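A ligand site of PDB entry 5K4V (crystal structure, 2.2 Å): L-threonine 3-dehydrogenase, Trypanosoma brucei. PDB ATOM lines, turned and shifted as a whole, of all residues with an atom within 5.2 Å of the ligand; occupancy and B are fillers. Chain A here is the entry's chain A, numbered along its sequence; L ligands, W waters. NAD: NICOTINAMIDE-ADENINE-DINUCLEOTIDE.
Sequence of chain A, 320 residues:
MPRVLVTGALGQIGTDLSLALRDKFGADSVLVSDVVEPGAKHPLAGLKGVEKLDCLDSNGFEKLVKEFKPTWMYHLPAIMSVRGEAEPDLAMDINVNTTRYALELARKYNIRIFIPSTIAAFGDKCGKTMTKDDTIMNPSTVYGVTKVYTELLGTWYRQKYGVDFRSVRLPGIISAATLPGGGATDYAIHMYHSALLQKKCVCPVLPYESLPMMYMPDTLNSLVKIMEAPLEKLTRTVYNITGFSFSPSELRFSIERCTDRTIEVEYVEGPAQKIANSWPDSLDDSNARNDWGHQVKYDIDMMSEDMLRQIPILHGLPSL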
ATOM      1  N   GLY A   8      -7.841  13.504 -23.624  1.00  0.00           N
ATOM      2  CA  GLY A   8      -6.471  13.794 -23.153  1.00  0.00           C
ATOM      3  C   GLY A   8      -6.051  12.778 -22.152  1.00  0.00           C
ATOM      4  O   GLY A   8      -5.413  13.088 -21.233  1.00  0.00           O
ATOM      5  N   ALA A   9      -6.414  11.523 -22.382  1.00  0.00           N
ATOM      6  CA  ALA A   9      -6.350  10.492 -21.409  1.00  0.00           C
ATOM      7  C   ALA A   9      -4.994   9.877 -21.090  1.00  0.00           C
ATOM      8  O   ALA A   9      -4.889   9.203 -20.064  1.00  0.00           O
ATOM      9  CB  ALA A   9      -7.293   9.368 -21.827  1.00  0.00           C
ATOM     10  N   LEU A  10      -3.983  10.089 -21.958  1.00  0.00           N
ATOM     11  CA  LEU A  10      -2.684   9.457 -21.809  1.00  0.00           C
ATOM     12  C   LEU A  10      -1.750  10.273 -20.977  1.00  0.00           C
ATOM     13  O   LEU A  10      -0.706   9.780 -20.642  1.00  0.00           O
ATOM     14  CB  LEU A  10      -2.015   9.243 -23.156  1.00  0.00           C
ATOM     15  CG  LEU A  10      -2.830   8.355 -24.088  1.00  0.00           C
ATOM     16  CD1 LEU A  10      -2.055   8.026 -25.367  1.00  0.00           C
ATOM     17  CD2 LEU A  10      -3.290   7.078 -23.411  1.00  0.00           C
ATOM     18  N   GLY A  11      -2.127  11.490 -20.632  1.00  0.00           N
ATOM     19  CA  GLY A  11      -1.347  12.324 -19.729  1.00  0.00           C
ATOM     20  C   GLY A  11      -1.232  11.878 -18.264  1.00  0.00           C
ATOM     21  O   GLY A  11      -1.650  10.785 -17.898  1.00  0.00           O
ATOM     22  N   GLN A  12      -0.691  12.767 -17.455  1.00  0.00           N
ATOM     23  CA  GLN A  12      -0.427  12.495 -16.047  1.00  0.00           C
ATOM     24  C   GLN A  12      -1.688  12.147 -15.302  1.00  0.00           C
ATOM     25  O   GLN A  12      -1.739  11.136 -14.587  1.00  0.00           O
ATOM     26  CB  GLN A  12       0.225  13.695 -15.382  1.00  0.00           C
ATOM     27  CG  GLN A  12       0.805  13.285 -14.054  1.00  0.00           C
ATOM     28  CD  GLN A  12       1.138  14.458 -13.140  1.00  0.00           C
ATOM     29  OE1 GLN A  12       1.355  15.602 -13.575  1.00  0.00           O
ATOM     30  NE2 GLN A  12       1.245  14.151 -11.856  1.00  0.00           N
ATOM     31  N   ILE A  13      -2.731  12.954 -15.494  1.00  0.00           N
ATOM     32  CA  ILE A  13      -3.958  12.765 -14.728  1.00  0.00           C
ATOM     33  C   ILE A  13      -4.789  11.706 -15.395  1.00  0.00           C
ATOM     34  O   ILE A  13      -5.396  10.892 -14.728  1.00  0.00           O
ATOM     35  CB  ILE A  13      -4.740  14.096 -14.619  1.00  0.00           C
ATOM     36  CG1 ILE A  13      -3.851  15.122 -13.852  1.00  0.00           C
ATOM     37  CG2 ILE A  13      -6.092  13.890 -13.953  1.00  0.00           C
ATOM     38  CD1 ILE A  13      -4.571  16.342 -13.342  1.00  0.00           C
ATOM     39  N   GLY A  14      -4.876  11.727 -16.735  1.00  0.00           N
ATOM     40  CA  GLY A  14      -5.764  10.825 -17.426  1.00  0.00           C
ATOM     41  C   GLY A  14      -5.381   9.370 -17.281  1.00  0.00           C
ATOM     42  O   GLY A  14      -6.236   8.488 -17.227  1.00  0.00           O
ATOM     43  N   ASP A  34      -7.147  10.218 -26.866  1.00  0.00           N
ATOM     44  CA  ASP A  34      -6.025  11.113 -26.858  1.00  0.00           C
ATOM     45  C   ASP A  34      -5.561  11.363 -28.276  1.00  0.00           C
ATOM     46  O   ASP A  34      -5.890  10.604 -29.162  1.00  0.00           O
ATOM     47  CB  ASP A  34      -4.900  10.543 -25.997  1.00  0.00           C
ATOM     48  CG  ASP A  34      -3.955  11.597 -25.493  1.00  0.00           C
ATOM     49  OD1 ASP A  34      -3.171  12.105 -26.324  1.00  0.00           O
ATOM     50  OD2 ASP A  34      -3.946  11.833 -24.247  1.00  0.00           O
ATOM     51  N   VAL A  35      -4.815  12.450 -28.479  1.00  0.00           N
ATOM     52  CA  VAL A  35      -4.350  12.829 -29.808  1.00  0.00           C
ATOM     53  C   VAL A  35      -3.328  11.834 -30.339  1.00  0.00           C
ATOM     54  O   VAL A  35      -3.158  11.718 -31.556  1.00  0.00           O
ATOM     55  CB  VAL A  35      -3.786  14.296 -29.850  1.00  0.00           C
ATOM     56  CG1 VAL A  35      -2.437  14.439 -29.116  1.00  0.00           C
ATOM     57  CG2 VAL A  35      -3.653  14.801 -31.290  1.00  0.00           C
ATOM     58  N   VAL A  36      -2.672  11.100 -29.438  1.00  0.00           N
ATOM     59  CA  VAL A  36      -1.703  10.043 -29.808  1.00  0.00           C
ATOM     60  C   VAL A  36      -2.090   8.694 -29.254  1.00  0.00           C
ATOM     61  O   VAL A  36      -3.084   8.585 -28.496  1.00  0.00           O
ATOM     62  CB  VAL A  36      -0.269  10.411 -29.396  1.00  0.00           C
ATOM     63  CG1 VAL A  36       0.183  11.629 -30.186  1.00  0.00           C
ATOM     64  CG2 VAL A  36      -0.188  10.749 -27.910  1.00  0.00           C
ATOM     65  N   LEU A  53      -7.990  10.424 -31.025  1.00  0.00           N
ATOM     66  CA  LEU A  53      -8.915  11.507 -31.338  1.00  0.00           C
ATOM     67  C   LEU A  53      -8.151  12.763 -31.050  1.00  0.00           C
ATOM     68  O   LEU A  53      -7.636  12.966 -29.932  1.00  0.00           O
ATOM     69  CB  LEU A  53     -10.178  11.450 -30.430  1.00  0.00           C
ATOM     70  CG  LEU A  53     -11.069  12.710 -30.420  1.00  0.00           C
ATOM     71  CD1 LEU A  53     -11.851  12.940 -31.710  1.00  0.00           C
ATOM     72  CD2 LEU A  53     -12.034  12.754 -29.250  1.00  0.00           C
ATOM     73  N   ASP A  54      -8.046  13.596 -32.064  1.00  0.00           N
ATOM     74  CA  ASP A  54      -7.588  14.969 -31.867  1.00  0.00           C
ATOM     75  C   ASP A  54      -8.813  15.807 -31.511  1.00  0.00           C
ATOM     76  O   ASP A  54      -9.666  16.018 -32.333  1.00  0.00           O
ATOM     77  CB  ASP A  54      -6.921  15.509 -33.124  1.00  0.00           C
ATOM     78  CG  ASP A  54      -6.346  16.924 -32.908  1.00  0.00           C
ATOM     79  OD1 ASP A  54      -6.810  17.692 -32.004  1.00  0.00           O
ATOM     80  OD2 ASP A  54      -5.382  17.244 -33.646  1.00  0.00           O
ATOM     81  N   CYS A  55      -8.899  16.310 -30.279  1.00  0.00           N
ATOM     82  CA  CYS A  55     -10.066  17.168 -29.902  1.00  0.00           C
ATOM     83  C   CYS A  55     -10.162  18.480 -30.676  1.00  0.00           C
ATOM     84  O   CYS A  55     -11.211  19.150 -30.610  1.00  0.00           O
ATOM     85  CB  CYS A  55     -10.038  17.505 -28.423  1.00  0.00           C
ATOM     86  SG  CYS A  55     -10.397  16.124 -27.364  1.00  0.00           S
ATOM     87  N   LEU A  56      -9.099  18.894 -31.373  1.00  0.00           N
ATOM     88  CA  LEU A  56      -9.241  20.043 -32.289  1.00  0.00           C
ATOM     89  C   LEU A  56      -9.988  19.667 -33.558  1.00  0.00           C
ATOM     90  O   LEU A  56     -10.280  20.537 -34.338  1.00  0.00           O
ATOM     91  CB  LEU A  56      -7.903  20.632 -32.672  1.00  0.00           C
ATOM     92  CG  LEU A  56      -7.205  21.476 -31.610  1.00  0.00           C
ATOM     93  CD1 LEU A  56      -5.828  21.836 -32.136  1.00  0.00           C
ATOM     94  CD2 LEU A  56      -7.995  22.733 -31.342  1.00  0.00           C
ATOM     95  N   HIS A  75     -12.751  16.398 -19.548  1.00  0.00           N
ATOM     96  CA  HIS A  75     -12.018  16.956 -20.651  1.00  0.00           C
ATOM     97  C   HIS A  75     -10.671  17.468 -20.150  1.00  0.00           C
ATOM     98  O   HIS A  75     -10.557  18.571 -19.623  1.00  0.00           O
ATOM     99  CB  HIS A  75     -12.836  18.002 -21.407  1.00  0.00           C
ATOM    100  CG  HIS A  75     -12.133  18.619 -22.583  1.00  0.00           C
ATOM    101  ND1 HIS A  75     -11.907  17.948 -23.755  1.00  0.00           N
ATOM    102  CD2 HIS A  75     -11.598  19.852 -22.757  1.00  0.00           C
ATOM    103  CE1 HIS A  75     -11.238  18.720 -24.590  1.00  0.00           C
ATOM    104  NE2 HIS A  75     -11.062  19.897 -24.020  1.00  0.00           N
ATOM    105  N   LEU A  76      -9.654  16.638 -20.351  1.00  0.00           N
ATOM    106  CA  LEU A  76      -8.346  16.836 -19.767  1.00  0.00           C
ATOM    107  C   LEU A  76      -7.250  17.453 -20.651  1.00  0.00           C
ATOM    108  O   LEU A  76      -6.260  17.861 -20.107  1.00  0.00           O
ATOM    109  CB  LEU A  76      -7.855  15.525 -19.183  1.00  0.00           C
ATOM    110  CG  LEU A  76      -8.803  14.864 -18.179  1.00  0.00           C
ATOM    111  CD1 LEU A  76      -8.172  13.633 -17.579  1.00  0.00           C
ATOM    112  CD2 LEU A  76      -9.111  15.827 -17.079  1.00  0.00           C
ATOM    113  N   PRO A  77      -7.443  17.574 -21.982  1.00  0.00           N
ATOM    114  CA  PRO A  77      -6.342  18.158 -22.773  1.00  0.00           C
ATOM    115  C   PRO A  77      -6.016  19.622 -22.429  1.00  0.00           C
ATOM    116  O   PRO A  77      -6.904  20.498 -22.397  1.00  0.00           O
ATOM    117  CB  PRO A  77      -6.836  18.057 -24.256  1.00  0.00           C
ATOM    118  CG  PRO A  77      -8.291  17.912 -24.178  1.00  0.00           C
ATOM    119  CD  PRO A  77      -8.624  17.285 -22.837  1.00  0.00           C
ATOM    120  N   ALA A  78      -4.726  19.863 -22.262  1.00  0.00           N
ATOM    121  CA  ALA A  78      -4.199  21.205 -22.004  1.00  0.00           C
ATOM    122  C   ALA A  78      -2.676  21.199 -22.199  1.00  0.00           C
ATOM    123  O   ALA A  78      -1.988  20.236 -21.839  1.00  0.00           O
ATOM    124  CB  ALA A  78      -4.543  21.659 -20.583  1.00  0.00           C
ATOM    125  N   ILE A  79      -2.170  22.279 -22.785  1.00  0.00           N
ATOM    126  CA  ILE A  79      -0.788  22.656 -22.736  1.00  0.00           C
ATOM    127  C   ILE A  79      -0.571  23.437 -21.454  1.00  0.00           C
ATOM    128  O   ILE A  79      -1.299  24.380 -21.143  1.00  0.00           O
ATOM    129  CB  ILE A  79      -0.444  23.604 -23.891  1.00  0.00           C
ATOM    130  CG1 ILE A  79      -0.787  22.935 -25.230  1.00  0.00           C
ATOM    131  CG2 ILE A  79       0.998  24.044 -23.754  1.00  0.00           C
ATOM    132  CD1 ILE A  79      -0.266  21.496 -25.358  1.00  0.00           C
ATOM    133  N   MET A  80       0.450  23.075 -20.719  1.00  0.00           N
ATOM    134  CA  MET A  80       0.553  23.493 -19.340  1.00  0.00           C
ATOM    135  C   MET A  80       1.478  24.681 -19.139  1.00  0.00           C
ATOM    136  O   MET A  80       1.880  25.300 -20.104  1.00  0.00           O
ATOM    137  CB  MET A  80       0.859  22.280 -18.489  1.00  0.00           C
ATOM    138  CG  MET A  80      -0.427  21.459 -18.257  1.00  0.00           C
ATOM    139  SD  MET A  80      -0.064  20.203 -17.067  1.00  0.00           S
ATOM    140  CE  MET A  80      -0.190  21.126 -15.552  1.00  0.00           C
ATOM    141  N   ILE A  94      -5.330  24.698 -28.055  1.00  0.00           N
ATOM    142  CA  ILE A  94      -5.837  23.572 -27.307  1.00  0.00           C
ATOM    143  C   ILE A  94      -6.722  23.996 -26.110  1.00  0.00           C
ATOM    144  O   ILE A  94      -7.819  23.471 -25.938  1.00  0.00           O
ATOM    145  CB  ILE A  94      -4.690  22.682 -26.797  1.00  0.00           C
ATOM    146  CG1 ILE A  94      -3.812  22.159 -27.957  1.00  0.00           C
ATOM    147  CG2 ILE A  94      -5.219  21.588 -25.893  1.00  0.00           C
ATOM    148  CD1 ILE A  94      -4.466  21.163 -28.871  1.00  0.00           C
ATOM    149  N   THR A  98     -10.429  23.395 -27.837  1.00  0.00           N
ATOM    150  CA  THR A  98     -10.954  22.068 -27.495  1.00  0.00           C
ATOM    151  C   THR A  98     -12.041  22.226 -26.407  1.00  0.00           C
ATOM    152  O   THR A  98     -13.019  21.485 -26.417  1.00  0.00           O
ATOM    153  CB  THR A  98      -9.861  21.036 -27.106  1.00  0.00           C
ATOM    154  OG1 THR A  98      -9.326  21.270 -25.786  1.00  0.00           O
ATOM    155  CG2 THR A  98      -8.678  21.027 -28.162  1.00  0.00           C
ATOM    156  N   PRO A 116     -10.872  20.710 -15.701  1.00  0.00           N
ATOM    157  CA  PRO A 116     -10.117  21.199 -14.546  1.00  0.00           C
ATOM    158  C   PRO A 116      -9.632  22.622 -14.730  1.00  0.00           C
ATOM    159  O   PRO A 116      -9.147  22.999 -15.817  1.00  0.00           O
ATOM    160  CB  PRO A 116      -8.891  20.257 -14.480  1.00  0.00           C
ATOM    161  CG  PRO A 116      -8.753  19.704 -15.853  1.00  0.00           C
ATOM    162  CD  PRO A 116     -10.151  19.662 -16.446  1.00  0.00           C
ATOM    163  N   SER A 117      -9.725  23.420 -13.687  1.00  0.00           N
ATOM    164  CA  SER A 117      -8.935  24.655 -13.670  1.00  0.00           C
ATOM    165  C   SER A 117      -7.652  24.307 -12.928  1.00  0.00           C
ATOM    166  O   SER A 117      -7.301  23.132 -12.803  1.00  0.00           O
ATOM    167  CB  SER A 117      -9.687  25.794 -13.013  1.00  0.00           C
ATOM    168  OG  SER A 117      -9.023  27.064 -13.221  1.00  0.00           O
ATOM    169  N   THR A 118      -6.999  25.322 -12.388  1.00  0.00           N
ATOM    170  CA  THR A 118      -5.703  25.190 -11.784  1.00  0.00           C
ATOM    171  C   THR A 118      -5.387  26.393 -10.900  1.00  0.00           C
ATOM    172  O   THR A 118      -5.925  27.475 -11.090  1.00  0.00           O
ATOM    173  CB  THR A 118      -4.612  25.129 -12.885  1.00  0.00           C
ATOM    174  OG1 THR A 118      -3.337  25.396 -12.325  1.00  0.00           O
ATOM    175  CG2 THR A 118      -4.843  26.203 -13.922  1.00  0.00           C
ATOM    176  N   TYR A 143      -1.343  30.086 -20.079  1.00  0.00           N
ATOM    177  CA  TYR A 143      -2.072  28.930 -19.557  1.00  0.00           C
ATOM    178  C   TYR A 143      -3.139  29.334 -18.490  1.00  0.00           C
ATOM    179  O   TYR A 143      -4.303  28.988 -18.586  1.00  0.00           O
ATOM    180  CB  TYR A 143      -1.043  27.977 -19.002  1.00  0.00           C
ATOM    181  CG  TYR A 143      -1.548  26.867 -18.137  1.00  0.00           C
ATOM    182  CD1 TYR A 143      -2.324  25.873 -18.655  1.00  0.00           C
ATOM    183  CD2 TYR A 143      -1.172  26.791 -16.774  1.00  0.00           C
ATOM    184  CE1 TYR A 143      -2.759  24.823 -17.833  1.00  0.00           C
ATOM    185  CE2 TYR A 143      -1.603  25.743 -15.977  1.00  0.00           C
ATOM    186  CZ  TYR A 143      -2.364  24.755 -16.513  1.00  0.00           C
ATOM    187  OH  TYR A 143      -2.791  23.665 -15.751  1.00  0.00           O
ATOM    188  N   LYS A 147      -7.167  29.269 -18.593  1.00  0.00           N
ATOM    189  CA  LYS A 147      -7.907  28.584 -17.517  1.00  0.00           C
ATOM    190  C   LYS A 147      -9.000  29.436 -16.857  1.00  0.00           C
ATOM    191  O   LYS A 147     -10.074  28.938 -16.519  1.00  0.00           O
ATOM    192  CB  LYS A 147      -6.962  27.968 -16.493  1.00  0.00           C
ATOM    193  CG  LYS A 147      -6.248  26.744 -17.025  1.00  0.00           C
ATOM    194  CD  LYS A 147      -7.269  25.672 -17.528  1.00  0.00           C
ATOM    195  CE  LYS A 147      -6.698  24.249 -17.586  1.00  0.00           C
ATOM    196  NZ  LYS A 147      -7.595  23.300 -18.365  1.00  0.00           N
ATOM    197  N   LEU A 170      -7.156  22.578  -9.598  1.00  0.00           N
ATOM    198  CA  LEU A 170      -6.142  21.590  -9.159  1.00  0.00           C
ATOM    199  C   LEU A 170      -4.874  22.293  -8.675  1.00  0.00           C
ATOM    200  O   LEU A 170      -4.438  23.283  -9.282  1.00  0.00           O
ATOM    201  CB  LEU A 170      -5.770  20.589 -10.266  1.00  0.00           C
ATOM    202  CG  LEU A 170      -6.868  19.598 -10.596  1.00  0.00           C
ATOM    203  CD1 LEU A 170      -6.554  18.773 -11.838  1.00  0.00           C
ATOM    204  CD2 LEU A 170      -7.186  18.714  -9.416  1.00  0.00           C
ATOM    205  N   PRO A 171      -4.327  21.821  -7.575  1.00  0.00           N
ATOM    206  CA  PRO A 171      -3.026  22.270  -7.122  1.00  0.00           C
ATOM    207  C   PRO A 171      -1.981  21.475  -7.916  1.00  0.00           C
ATOM    208  O   PRO A 171      -2.380  20.726  -8.798  1.00  0.00           O
ATOM    209  CB  PRO A 171      -3.032  21.869  -5.653  1.00  0.00           C
ATOM    210  CG  PRO A 171      -3.800  20.630  -5.614  1.00  0.00           C
ATOM    211  CD  PRO A 171      -4.871  20.798  -6.680  1.00  0.00           C
ATOM    212  N   GLY A 172      -0.709  21.579  -7.600  1.00  0.00           N
ATOM    213  CA  GLY A 172       0.285  20.647  -8.159  1.00  0.00           C
ATOM    214  C   GLY A 172      -0.057  19.165  -7.832  1.00  0.00           C
ATOM    215  O   GLY A 172      -0.261  18.795  -6.657  1.00  0.00           O
ATOM    216  N   ILE A 173      -0.157  18.320  -8.867  1.00  0.00           N
ATOM    217  CA  ILE A 173      -0.478  16.890  -8.666  1.00  0.00           C
ATOM    218  C   ILE A 173       0.773  16.011  -8.770  1.00  0.00           C
ATOM    219  O   ILE A 173       1.508  16.092  -9.746  1.00  0.00           O
ATOM    220  CB  ILE A 173      -1.535  16.395  -9.668  1.00  0.00           C
ATOM    221  CG1 ILE A 173      -2.782  17.301  -9.686  1.00  0.00           C
ATOM    222  CG2 ILE A 173      -1.925  14.956  -9.353  1.00  0.00           C
ATOM    223  CD1 ILE A 173      -3.519  17.387  -8.358  1.00  0.00           C
ATOM    224  N   LEU A 179       4.612  10.523 -16.501  1.00  0.00           N
ATOM    225  CA  LEU A 179       5.410  11.729 -16.299  1.00  0.00           C
ATOM    226  C   LEU A 179       4.629  12.971 -16.717  1.00  0.00           C
ATOM    227  O   LEU A 179       3.822  12.931 -17.634  1.00  0.00           O
ATOM    228  CB  LEU A 179       6.731  11.649 -17.097  1.00  0.00           C
ATOM    229  CG  LEU A 179       7.702  10.540 -16.665  1.00  0.00           C
ATOM    230  CD1 LEU A 179       8.723  10.300 -17.784  1.00  0.00           C
ATOM    231  CD2 LEU A 179       8.362  10.897 -15.355  1.00  0.00           C
ATOM    232  N   PRO A 180       4.866  14.073 -16.012  1.00  0.00           N
ATOM    233  CA  PRO A 180       4.097  15.325 -16.146  1.00  0.00           C
ATOM    234  C   PRO A 180       4.359  16.017 -17.447  1.00  0.00           C
ATOM    235  O   PRO A 180       5.470  15.901 -17.962  1.00  0.00           O
ATOM    236  CB  PRO A 180       4.681  16.198 -15.019  1.00  0.00           C
ATOM    237  CG  PRO A 180       6.087  15.678 -14.805  1.00  0.00           C
ATOM    238  CD  PRO A 180       5.950  14.179 -15.002  1.00  0.00           C
ATOM    239  N   GLY A 181       3.348  16.700 -17.995  1.00  0.00           N
ATOM    240  CA  GLY A 181       3.495  17.543 -19.201  1.00  0.00           C
ATOM    241  C   GLY A 181       4.470  18.675 -18.935  1.00  0.00           C
ATOM    242  O   GLY A 181       5.423  18.535 -18.193  1.00  0.00           O
ATOM    243  N   GLY A 182       4.310  19.828 -19.519  1.00  0.00           N
ATOM    244  CA  GLY A 182       5.317  20.865 -19.132  1.00  0.00           C
ATOM    245  C   GLY A 182       4.880  21.850 -18.064  1.00  0.00           C
ATOM    246  O   GLY A 182       4.617  23.007 -18.377  1.00  0.00           O
ATOM    247  N   THR A 185       5.301  22.664 -11.436  1.00  0.00           N
ATOM    248  CA  THR A 185       5.398  21.704 -10.326  1.00  0.00           C
ATOM    249  C   THR A 185       6.054  20.368 -10.705  1.00  0.00           C
ATOM    250  O   THR A 185       6.168  19.469  -9.864  1.00  0.00           O
ATOM    251  CB  THR A 185       4.009  21.415  -9.684  1.00  0.00           C
ATOM    252  OG1 THR A 185       3.194  20.710 -10.607  1.00  0.00           O
ATOM    253  CG2 THR A 185       3.280  22.717  -9.367  1.00  0.00           C
HETATM  254  PA  NAD L   1      -0.379  16.159 -19.617  1.00  0.00           P
HETATM  255  O1A NAD L   1       0.251  15.147 -18.666  1.00  0.00           O
HETATM  256  O2A NAD L   1       0.437  17.093 -20.466  1.00  0.00           O
HETATM  257  O5B NAD L   1      -1.254  15.401 -20.717  1.00  0.00           O
HETATM  258  C5B NAD L   1      -2.124  16.191 -21.565  1.00  0.00           C
HETATM  259  C4B NAD L   1      -2.820  15.214 -22.488  1.00  0.00           C
HETATM  260  O4B NAD L   1      -3.681  15.902 -23.490  1.00  0.00           O
HETATM  261  C3B NAD L   1      -1.660  14.525 -23.246  1.00  0.00           C
HETATM  262  O3B NAD L   1      -1.906  13.116 -23.273  1.00  0.00           O
HETATM  263  C2B NAD L   1      -1.838  15.148 -24.636  1.00  0.00           C
HETATM  264  O2B NAD L   1      -1.426  14.261 -25.679  1.00  0.00           O
HETATM  265  C1B NAD L   1      -3.356  15.291 -24.698  1.00  0.00           C
HETATM  266  N9A NAD L   1      -3.611  16.248 -25.752  1.00  0.00           N
HETATM  267  C8A NAD L   1      -2.911  17.348 -26.100  1.00  0.00           C
HETATM  268  N7A NAD L   1      -3.522  17.930 -27.118  1.00  0.00           N
HETATM  269  C5A NAD L   1      -4.612  17.200 -27.435  1.00  0.00           C
HETATM  270  C6A NAD L   1      -5.594  17.291 -28.404  1.00  0.00           C
HETATM  271  N6A NAD L   1      -5.596  18.288 -29.267  1.00  0.00           N
HETATM  272  N1A NAD L   1      -6.552  16.359 -28.458  1.00  0.00           N
HETATM  273  C2A NAD L   1      -6.551  15.362 -27.595  1.00  0.00           C
HETATM  274  N3A NAD L   1      -5.624  15.208 -26.659  1.00  0.00           N
HETATM  275  C4A NAD L   1      -4.644  16.123 -26.574  1.00  0.00           C
HETATM  276  O3  NAD L   1      -1.417  17.090 -18.738  1.00  0.00           O
HETATM  277  PN  NAD L   1      -2.051  16.579 -17.284  1.00  0.00           P
HETATM  278  O1N NAD L   1      -2.605  15.209 -17.420  1.00  0.00           O
HETATM  279  O2N NAD L   1      -1.132  16.861 -16.159  1.00  0.00           O
HETATM  280  O5D NAD L   1      -3.229  17.681 -17.245  1.00  0.00           O
HETATM  281  C5D NAD L   1      -4.571  17.320 -17.598  1.00  0.00           C
HETATM  282  C4D NAD L   1      -5.544  18.451 -17.232  1.00  0.00           C
HETATM  283  O4D NAD L   1      -5.437  18.624 -15.833  1.00  0.00           O
HETATM  284  C3D NAD L   1      -5.159  19.802 -17.864  1.00  0.00           C
HETATM  285  O3D NAD L   1      -6.339  20.601 -18.137  1.00  0.00           O
HETATM  286  C2D NAD L   1      -4.256  20.457 -16.825  1.00  0.00           C
HETATM  287  O2D NAD L   1      -4.274  21.874 -16.994  1.00  0.00           O
HETATM  288  C1D NAD L   1      -4.982  20.019 -15.560  1.00  0.00           C
HETATM  289  N1N NAD L   1      -4.062  20.170 -14.375  1.00  0.00           N
HETATM  290  C2N NAD L   1      -2.988  19.270 -14.140  1.00  0.00           C
HETATM  291  C3N NAD L   1      -2.163  19.466 -13.022  1.00  0.00           C
HETATM  292  C7N NAD L   1      -1.005  18.534 -12.758  1.00  0.00           C
HETATM  293  O7N NAD L   1      -0.053  18.934 -11.852  1.00  0.00           O
HETATM  294  N7N NAD L   1      -0.974  17.372 -13.477  1.00  0.00           N
HETATM  295  C4N NAD L   1      -2.365  20.552 -12.143  1.00  0.00           C
HETATM  296  C5N NAD L   1      -3.416  21.402 -12.378  1.00  0.00           C
HETATM  297  C6N NAD L   1      -4.280  21.250 -13.477  1.00  0.00           C
HETATM  298  O   HOH W   1       2.472  18.191 -11.529  1.00  0.00           O
HETATM  299  O   HOH W   2       1.512  16.988 -15.747  1.00  0.00           O
HETATM  300  O   HOH W   3      -9.034  13.094 -27.109  1.00  0.00           O
HETATM  301  O   HOH W   4       2.617  14.292 -19.575  1.00  0.00           O
HETATM  302  O   HOH W   5      -8.384  20.404 -19.837  1.00  0.00           O
HETATM  303  O   HOH W   6      -4.065  13.542 -18.782  1.00  0.00           O
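Water W6 lies within hydrogen-bond range of an oxygen (O1N) of the ligand (2.6 Å), the backbone carbonyl oxygen (O) of Gly 8 (2.8 Å), the backbone NH (N) of Gly 14 (2.9 Å) and the backbone NH (N) of Gly 11 (3.4 Å).
Water W4 lies within hydrogen-bond range of O of Leu 179 (2.7 Å), O1A of the ligand (2.7 Å) and N of Gly 181 (3.0 Å).
Water W2 lies within hydrogen-bond range of the side-chain amide oxygen (OE1) of Gln 12, an oxygen (O2N) of the ligand and the backbone NH (N) of Gly 181.
Water W3 lies within hydrogen-bond range of O of Leu 53 (3.2 Å), SG of Cys 55 (3.3 Å) and N of Asp 34 (3.4 Å).
O2N of the ligand sits close to SD of Met 80 (3.6 Å).
Gly 8 touches the ligand.
C of Leu 10 touches O3B of the ligand, 3.7 Å away.
Leu 53 touches the ligand.
CA of Pro 77 touches O4B of the ligand, 3.6 Å away.
Ala 78 touches the ligand.
Ile 94 touches the ligand (CD1 to N6A, 3.1 Å).
CG of Pro 116 touches O3D of the ligand, at 3.4 Å.
O of Ser 117 touches C6N of the ligand, 3.6 Å away.
Thr 118 touches the ligand (CB to C6N, 3.9 Å).
CB of Leu 170 touches C5N of the ligand, 3.3 Å away.
O of Pro 171 touches C4N of the ligand, at 3.3 Å.
CA of Gly 181 touches O2A of the ligand, 3.3 Å away.
Thr 185 touches the ligand (OG1 to O7N, 3.9 Å).
Hydrophobic or aromatic side chains that line the ligand: Leu 10, Ile 13, Val 35, Pro 77, Ala 78, Met 80, Ile 94, Pro 116, Tyr 143, Leu 170 and Ile 173.
Within 4 Å of the ligand: Gly 8, Leu 10, Gly 11, Gln 12, Ile 13, Asp 34, Val 35, Leu 53, Asp 54, Cys 55, Leu 76, Pro 77, Ala 78, Met 80, Ile 94, Pro 116, Ser 117, Thr 118, Tyr 143, Lys 147, Leu 170, Pro 171, Ile 173, Gly 181 and Thr 185.
The nearest printed residue that does not touch the ligand is Gly 172 (4.03 Å).
The side-chain carboxylate (OD2) of Asp 34 is in hydrogen-bond range of an oxygen (O3B) of the ligand, 2.6 Å away.
The side-chain hydroxyl of Tyr 143 lies within hydrogen-bond range of an oxygen (O2D) of the ligand, at 2.6 Å.
The backbone NH of Gln 12 lies within hydrogen-bond range of an oxygen (O1A) of the ligand (2.8 Å).
The side-chain amide oxygen of Gln 12 sits at hydrogen-bond distance from a nitrogen (N7N) of the ligand.
The backbone NH (N) of Ile 13 sits at hydrogen-bond distance from an oxygen (O1N) of the ligand, 3.0 Å away.
The backbone NH of Cys 55 lies within hydrogen-bond range of a nitrogen (N1A) of the ligand.
NZ of Lys 147 lies within hydrogen-bond range of O3D of the ligand, 3.0 Å away.
The backbone carbonyl oxygen of Leu 76 lies close to an oxygen (O3D) of the ligand, 3.4 Å away.
The backbone NH (N) of Ile 173 sits at hydrogen-bond distance from an oxygen (O7N) of the ligand, 3.0 Å away.
A nitrogen (N6A) of the ligand is in hydrogen-bond range of the side-chain carboxylate (OD1) of Asp 54 (3.1 Å).
N of Gly 11 lies within hydrogen-bond range of O3B of the ligand, 3.1 Å away.
The backbone NH (N) of Val 35 sits at hydrogen-bond distance from a nitrogen (N3A) of the ligand, at 3.4 Å.
The backbone NH (N) of Leu 53 is in hydrogen-bond range of the backbone carbonyl oxygen (O) of Asp 34 (2.8 Å).
The side-chain carboxylate of Asp 34 is in hydrogen-bond range of the backbone NH of Leu 10 (2.9 Å).
The side-chain carboxylate of Asp 34 sits close to the backbone NH of Val 36, 3.3 Å away.
The side-chain carboxylate (OD2) of Asp 34 lies within hydrogen-bond range of the backbone NH (N) of Ala 9 (3.1 Å).
The backbone carbonyl oxygen (O) of Ile 173 sits at hydrogen-bond distance from the side-chain amide nitrogen (NE2) of Gln 12 (2.9 Å).
The side-chain amino group (NZ) of Lys 147 is in hydrogen-bond range of the backbone carbonyl oxygen (O) of Pro 116 (3.0 Å).
The side-chain carboxylate (OD1) of Asp 54 is in hydrogen-bond range of the backbone NH (N) of Leu 56 (2.7 Å).
The side-chain hydroxyl (OG1) of Thr 98 is in hydrogen-bond range of the backbone carbonyl oxygen (O) of Ile 94 (2.7 Å).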
